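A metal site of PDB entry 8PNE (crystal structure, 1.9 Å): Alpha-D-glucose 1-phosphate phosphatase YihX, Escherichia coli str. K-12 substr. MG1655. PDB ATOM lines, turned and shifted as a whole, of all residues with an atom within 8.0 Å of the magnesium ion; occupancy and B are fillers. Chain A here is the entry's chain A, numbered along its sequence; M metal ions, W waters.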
ATOM      1  N   PHE A   5      23.473 -14.594 -19.343  1.00  0.00           N
ATOM      2  CA  PHE A   5      22.888 -15.212 -18.165  1.00  0.00           C
ATOM      3  C   PHE A   5      23.971 -15.911 -17.360  1.00  0.00           C
ATOM      4  O   PHE A   5      24.709 -16.697 -17.921  1.00  0.00           O
ATOM      5  CB  PHE A   5      21.871 -16.274 -18.575  1.00  0.00           C
ATOM      6  CG  PHE A   5      20.645 -15.751 -19.287  1.00  0.00           C
ATOM      7  CD1 PHE A   5      19.546 -15.331 -18.575  1.00  0.00           C
ATOM      8  CD2 PHE A   5      20.601 -15.681 -20.666  1.00  0.00           C
ATOM      9  CE1 PHE A   5      18.410 -14.867 -19.228  1.00  0.00           C
ATOM     10  CE2 PHE A   5      19.472 -15.205 -21.323  1.00  0.00           C
ATOM     11  CZ  PHE A   5      18.383 -14.787 -20.597  1.00  0.00           C
ATOM     12  N   ASP A   6      24.026 -15.611 -16.063  1.00  0.00           N
ATOM     13  CA  ASP A   6      24.601 -16.462 -15.035  1.00  0.00           C
ATOM     14  C   ASP A   6      23.967 -17.840 -15.084  1.00  0.00           C
ATOM     15  O   ASP A   6      22.864 -18.006 -15.610  1.00  0.00           O
ATOM     16  CB  ASP A   6      24.332 -15.855 -13.659  1.00  0.00           C
ATOM     17  CG  ASP A   6      24.906 -16.569 -12.455  1.00  0.00           C
ATOM     18  OD1 ASP A   6      25.887 -17.309 -12.595  1.00  0.00           O
ATOM     19  OD2 ASP A   6      24.345 -16.379 -11.385  1.00  0.00           O
ATOM     20  N   LEU A   7      24.694 -18.847 -14.580  1.00  0.00           N
ATOM     21  CA  LEU A   7      24.199 -20.220 -14.571  1.00  0.00           C
ATOM     22  C   LEU A   7      23.568 -20.495 -13.196  1.00  0.00           C
ATOM     23  O   LEU A   7      22.364 -20.660 -13.056  1.00  0.00           O
ATOM     24  CB  LEU A   7      25.376 -21.121 -14.892  1.00  0.00           C
ATOM     25  CG  LEU A   7      25.111 -22.614 -15.056  1.00  0.00           C
ATOM     26  CD1 LEU A   7      23.936 -22.844 -15.954  1.00  0.00           C
ATOM     27  CD2 LEU A   7      26.340 -23.292 -15.613  1.00  0.00           C
ATOM     28  N   GLY A   8      24.387 -20.427 -12.166  1.00  0.00           N
ATOM     29  CA  GLY A   8      23.997 -20.768 -10.810  1.00  0.00           C
ATOM     30  C   GLY A   8      22.957 -19.803 -10.234  1.00  0.00           C
ATOM     31  O   GLY A   8      23.261 -18.597 -10.037  1.00  0.00           O
ATOM     32  N   ASN A   9      21.772 -20.402  -9.997  1.00  0.00           N
ATOM     33  CA  ASN A   9      20.652 -19.799  -9.290  1.00  0.00           C
ATOM     34  C   ASN A   9      20.014 -18.788 -10.231  1.00  0.00           C
ATOM     35  O   ASN A   9      19.348 -17.851  -9.786  1.00  0.00           O
ATOM     36  CB  ASN A   9      21.048 -19.262  -7.900  1.00  0.00           C
ATOM     37  CG  ASN A   9      19.874 -18.812  -7.027  1.00  0.00           C
ATOM     38  OD1 ASN A   9      18.815 -19.455  -6.975  1.00  0.00           O
ATOM     39  ND2 ASN A   9      20.063 -17.726  -6.293  1.00  0.00           N
ATOM     40  N   VAL A  10      20.108 -19.090 -11.527  1.00  0.00           N
ATOM     41  CA  VAL A  10      19.516 -18.270 -12.575  1.00  0.00           C
ATOM     42  C   VAL A  10      18.958 -19.173 -13.656  1.00  0.00           C
ATOM     43  O   VAL A  10      17.767 -19.107 -13.980  1.00  0.00           O
ATOM     44  CB  VAL A  10      20.527 -17.270 -13.157  1.00  0.00           C
ATOM     45  CG1 VAL A  10      20.079 -16.736 -14.515  1.00  0.00           C
ATOM     46  CG2 VAL A  10      20.814 -16.149 -12.191  1.00  0.00           C
ATOM     47  N   ILE A  11      19.808 -19.991 -14.263  1.00  0.00           N
ATOM     48  CA  ILE A  11      19.317 -20.981 -15.201  1.00  0.00           C
ATOM     49  C   ILE A  11      19.012 -22.307 -14.479  1.00  0.00           C
ATOM     50  O   ILE A  11      18.124 -23.046 -14.895  1.00  0.00           O
ATOM     51  CB  ILE A  11      20.316 -21.183 -16.339  1.00  0.00           C
ATOM     52  CG1 ILE A  11      20.530 -19.908 -17.171  1.00  0.00           C
ATOM     53  CG2 ILE A  11      19.925 -22.336 -17.227  1.00  0.00           C
ATOM     54  CD1 ILE A  11      21.717 -20.001 -18.107  1.00  0.00           C
ATOM     55  N   VAL A  12      19.816 -22.643 -13.453  1.00  0.00           N
ATOM     56  CA  VAL A  12      19.616 -23.837 -12.660  1.00  0.00           C
ATOM     57  C   VAL A  12      19.534 -23.456 -11.188  1.00  0.00           C
ATOM     58  O   VAL A  12      20.208 -22.527 -10.767  1.00  0.00           O
ATOM     59  CB  VAL A  12      20.757 -24.847 -12.858  1.00  0.00           C
ATOM     60  CG1 VAL A  12      20.913 -25.260 -14.321  1.00  0.00           C
ATOM     61  CG2 VAL A  12      22.056 -24.338 -12.263  1.00  0.00           C
ATOM     62  N   ILE A  14      20.943 -24.672  -7.707  1.00  0.00           N
ATOM     63  CA  ILE A  14      22.113 -25.431  -7.358  1.00  0.00           C
ATOM     64  C   ILE A  14      22.275 -25.363  -5.845  1.00  0.00           C
ATOM     65  O   ILE A  14      22.009 -24.318  -5.255  1.00  0.00           O
ATOM     66  CB  ILE A  14      23.336 -24.926  -8.140  1.00  0.00           C
ATOM     67  CG1 ILE A  14      24.581 -25.789  -7.917  1.00  0.00           C
ATOM     68  CG2 ILE A  14      23.639 -23.472  -7.843  1.00  0.00           C
ATOM     69  CD1 ILE A  14      25.603 -25.645  -9.007  1.00  0.00           C
ATOM     70  N   LEU A 106      27.498 -16.949 -18.739  1.00  0.00           N
ATOM     71  CA  LEU A 106      28.734 -16.562 -18.081  1.00  0.00           C
ATOM     72  C   LEU A 106      28.779 -17.125 -16.661  1.00  0.00           C
ATOM     73  O   LEU A 106      28.053 -16.681 -15.771  1.00  0.00           O
ATOM     74  CB  LEU A 106      28.838 -15.025 -18.076  1.00  0.00           C
ATOM     75  CG  LEU A 106      30.143 -14.484 -17.475  1.00  0.00           C
ATOM     76  CD1 LEU A 106      31.358 -15.026 -18.216  1.00  0.00           C
ATOM     77  CD2 LEU A 106      30.162 -12.971 -17.462  1.00  0.00           C
ATOM     78  N   SER A 107      29.744 -18.029 -16.423  1.00  0.00           N
ATOM     79  CA  SER A 107      29.752 -18.799 -15.200  1.00  0.00           C
ATOM     80  C   SER A 107      31.160 -18.945 -14.646  1.00  0.00           C
ATOM     81  O   SER A 107      32.062 -19.365 -15.354  1.00  0.00           O
ATOM     82  CB  SER A 107      29.140 -20.178 -15.414  1.00  0.00           C
ATOM     83  OG  SER A 107      29.342 -21.044 -14.308  1.00  0.00           O
ATOM     84  N   ASN A 108      31.280 -18.615 -13.371  1.00  0.00           N
ATOM     85  CA  ASN A 108      32.388 -19.030 -12.545  1.00  0.00           C
ATOM     86  C   ASN A 108      32.194 -20.477 -12.139  1.00  0.00           C
ATOM     87  O   ASN A 108      31.234 -20.795 -11.428  1.00  0.00           O
ATOM     88  CB  ASN A 108      32.447 -18.205 -11.262  1.00  0.00           C
ATOM     89  CG  ASN A 108      32.761 -16.749 -11.475  1.00  0.00           C
ATOM     90  OD1 ASN A 108      33.138 -16.320 -12.567  1.00  0.00           O
ATOM     91  ND2 ASN A 108      32.746 -15.996 -10.386  1.00  0.00           N
ATOM     92  N   LYS A 141      33.866 -13.602 -12.706  1.00  0.00           N
ATOM     93  CA  LYS A 141      33.043 -12.490 -12.199  1.00  0.00           C
ATOM     94  C   LYS A 141      33.405 -12.241 -10.733  1.00  0.00           C
ATOM     95  O   LYS A 141      33.786 -13.186 -10.050  1.00  0.00           O
ATOM     96  CB  LYS A 141      31.542 -12.813 -12.296  1.00  0.00           C
ATOM     97  CG  LYS A 141      31.086 -13.119 -13.715  1.00  0.00           C
ATOM     98  CD  LYS A 141      29.671 -13.628 -13.776  1.00  0.00           C
ATOM     99  CE  LYS A 141      29.500 -14.963 -13.072  1.00  0.00           C
ATOM    100  NZ  LYS A 141      28.136 -15.487 -13.318  1.00  0.00           N
ATOM    101  N   PHE A 164      21.971 -10.976 -16.474  1.00  0.00           N
ATOM    102  CA  PHE A 164      21.201 -11.520 -15.357  1.00  0.00           C
ATOM    103  C   PHE A 164      22.089 -12.320 -14.409  1.00  0.00           C
ATOM    104  O   PHE A 164      22.765 -13.258 -14.841  1.00  0.00           O
ATOM    105  CB  PHE A 164      20.109 -12.445 -15.901  1.00  0.00           C
ATOM    106  CG  PHE A 164      19.076 -11.723 -16.724  1.00  0.00           C
ATOM    107  CD1 PHE A 164      18.042 -11.042 -16.113  1.00  0.00           C
ATOM    108  CD2 PHE A 164      19.159 -11.694 -18.103  1.00  0.00           C
ATOM    109  CE1 PHE A 164      17.091 -10.370 -16.864  1.00  0.00           C
ATOM    110  CE2 PHE A 164      18.210 -11.018 -18.863  1.00  0.00           C
ATOM    111  CZ  PHE A 164      17.171 -10.366 -18.244  1.00  0.00           C
ATOM    112  N   ASP A 165      22.119 -11.927 -13.136  1.00  0.00           N
ATOM    113  CA  ASP A 165      22.872 -12.632 -12.121  1.00  0.00           C
ATOM    114  C   ASP A 165      22.250 -12.374 -10.754  1.00  0.00           C
ATOM    115  O   ASP A 165      21.640 -11.342 -10.510  1.00  0.00           O
ATOM    116  CB  ASP A 165      24.336 -12.256 -12.241  1.00  0.00           C
ATOM    117  CG  ASP A 165      25.328 -13.093 -11.449  1.00  0.00           C
ATOM    118  OD1 ASP A 165      25.121 -13.274 -10.236  1.00  0.00           O
ATOM    119  OD2 ASP A 165      26.359 -13.478 -12.053  1.00  0.00           O
ATOM    120  N   ASP A 166      22.374 -13.336  -9.843  1.00  0.00           N
ATOM    121  CA  ASP A 166      21.760 -13.231  -8.531  1.00  0.00           C
ATOM    122  C   ASP A 166      22.764 -12.668  -7.538  1.00  0.00           C
ATOM    123  O   ASP A 166      22.409 -12.472  -6.387  1.00  0.00           O
ATOM    124  CB  ASP A 166      21.238 -14.596  -8.035  1.00  0.00           C
ATOM    125  CG  ASP A 166      22.304 -15.671  -8.023  1.00  0.00           C
ATOM    126  OD1 ASP A 166      22.851 -15.966  -9.100  1.00  0.00           O
ATOM    127  OD2 ASP A 166      22.591 -16.193  -6.941  1.00  0.00           O
ATOM    128  N   ASN A 167      24.023 -12.497  -7.943  1.00  0.00           N
ATOM    129  CA  ASN A 167      25.034 -12.012  -7.040  1.00  0.00           C
ATOM    130  C   ASN A 167      25.212 -10.508  -7.232  1.00  0.00           C
ATOM    131  O   ASN A 167      25.427 -10.042  -8.348  1.00  0.00           O
ATOM    132  CB  ASN A 167      26.348 -12.727  -7.278  1.00  0.00           C
ATOM    133  CG  ASN A 167      27.474 -12.208  -6.425  1.00  0.00           C
ATOM    134  OD1 ASN A 167      28.008 -11.107  -6.613  1.00  0.00           O
ATOM    135  ND2 ASN A 167      27.872 -13.035  -5.490  1.00  0.00           N
ATOM    136  N   ASN A 170      28.421  -9.203  -8.641  1.00  0.00           N
ATOM    137  CA  ASN A 170      28.578  -9.489 -10.058  1.00  0.00           C
ATOM    138  C   ASN A 170      27.847  -8.401 -10.835  1.00  0.00           C
ATOM    139  O   ASN A 170      28.312  -7.957 -11.903  1.00  0.00           O
ATOM    140  CB  ASN A 170      28.046 -10.853 -10.468  1.00  0.00           C
ATOM    141  CG  ASN A 170      28.892 -12.015  -9.984  1.00  0.00           C
ATOM    142  OD1 ASN A 170      29.964 -11.822  -9.434  1.00  0.00           O
ATOM    143  ND2 ASN A 170      28.381 -13.219 -10.190  1.00  0.00           N
ATOM    144  N   VAL A 184      18.899 -10.986 -10.042  1.00  0.00           N
ATOM    145  CA  VAL A 184      17.881 -12.039 -10.013  1.00  0.00           C
ATOM    146  C   VAL A 184      17.508 -12.260  -8.552  1.00  0.00           C
ATOM    147  O   VAL A 184      18.344 -12.646  -7.744  1.00  0.00           O
ATOM    148  CB  VAL A 184      18.361 -13.293 -10.765  1.00  0.00           C
ATOM    149  CG1 VAL A 184      17.443 -14.493 -10.564  1.00  0.00           C
ATOM    150  CG2 VAL A 184      18.511 -12.999 -12.254  1.00  0.00           C
HETATM  151 MG    MG M   1      24.479 -17.060  -9.543  1.00  0.00          MG
HETATM  152  O   HOH W   1      25.920 -15.659  -9.231  1.00  0.00           O
HETATM  153  O   HOH W   2      25.947 -18.342 -10.066  1.00  0.00           O
HETATM  154  O   HOH W   3      24.436 -17.744  -7.668  1.00  0.00           O
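The side-chain carboxylate (OD1) of Asp 6 is in salt-bridge range of the side-chain amino group (NZ) of Lys 141 (3.0 Å).
O of Phe 164 is in hydrogen-bond range of N of Asp 6 (2.9 Å).
OD2 of Asp 166 lies within hydrogen-bond range of ND2 of Asn 9 (3.0 Å).
OD1 of Asp 165 lies within hydrogen-bond range of N of Asn 167, at 2.7 Å.
The side-chain carboxylate of Asp 165 lies within salt-bridge range of the side-chain amino group of Lys 141 (3.0 Å).
The side-chain amide nitrogen of Asn 170 sits at hydrogen-bond distance from the side-chain carboxylate of Asp 165, 2.8 Å away.
O of Asp 165 sits at hydrogen-bond distance from N of Val 184 (2.8 Å).
Asp 165 touches the magnesium ion (OD1 to MG, 3.9 Å).
Four residues have an atom within 4 Å of the magnesium ion: Asp 6, Gly 8, Asp 165 and Asp 166.
The magnesium ion is bound by the side-chain carboxylate of Asp 6 (2.0 Å), water W3 (2.0 Å), the side-chain carboxylate of Asp 166 (2.0 Å), water W2 (2.0 Å), the backbone carbonyl oxygen of Gly 8 (2.0 Å) and water W1 (2.0 Å).
Water W2 lies within hydrogen-bond range of the side-chain carboxylate (OD1) of Asp 6 and the backbone NH (N) of Gly 8.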
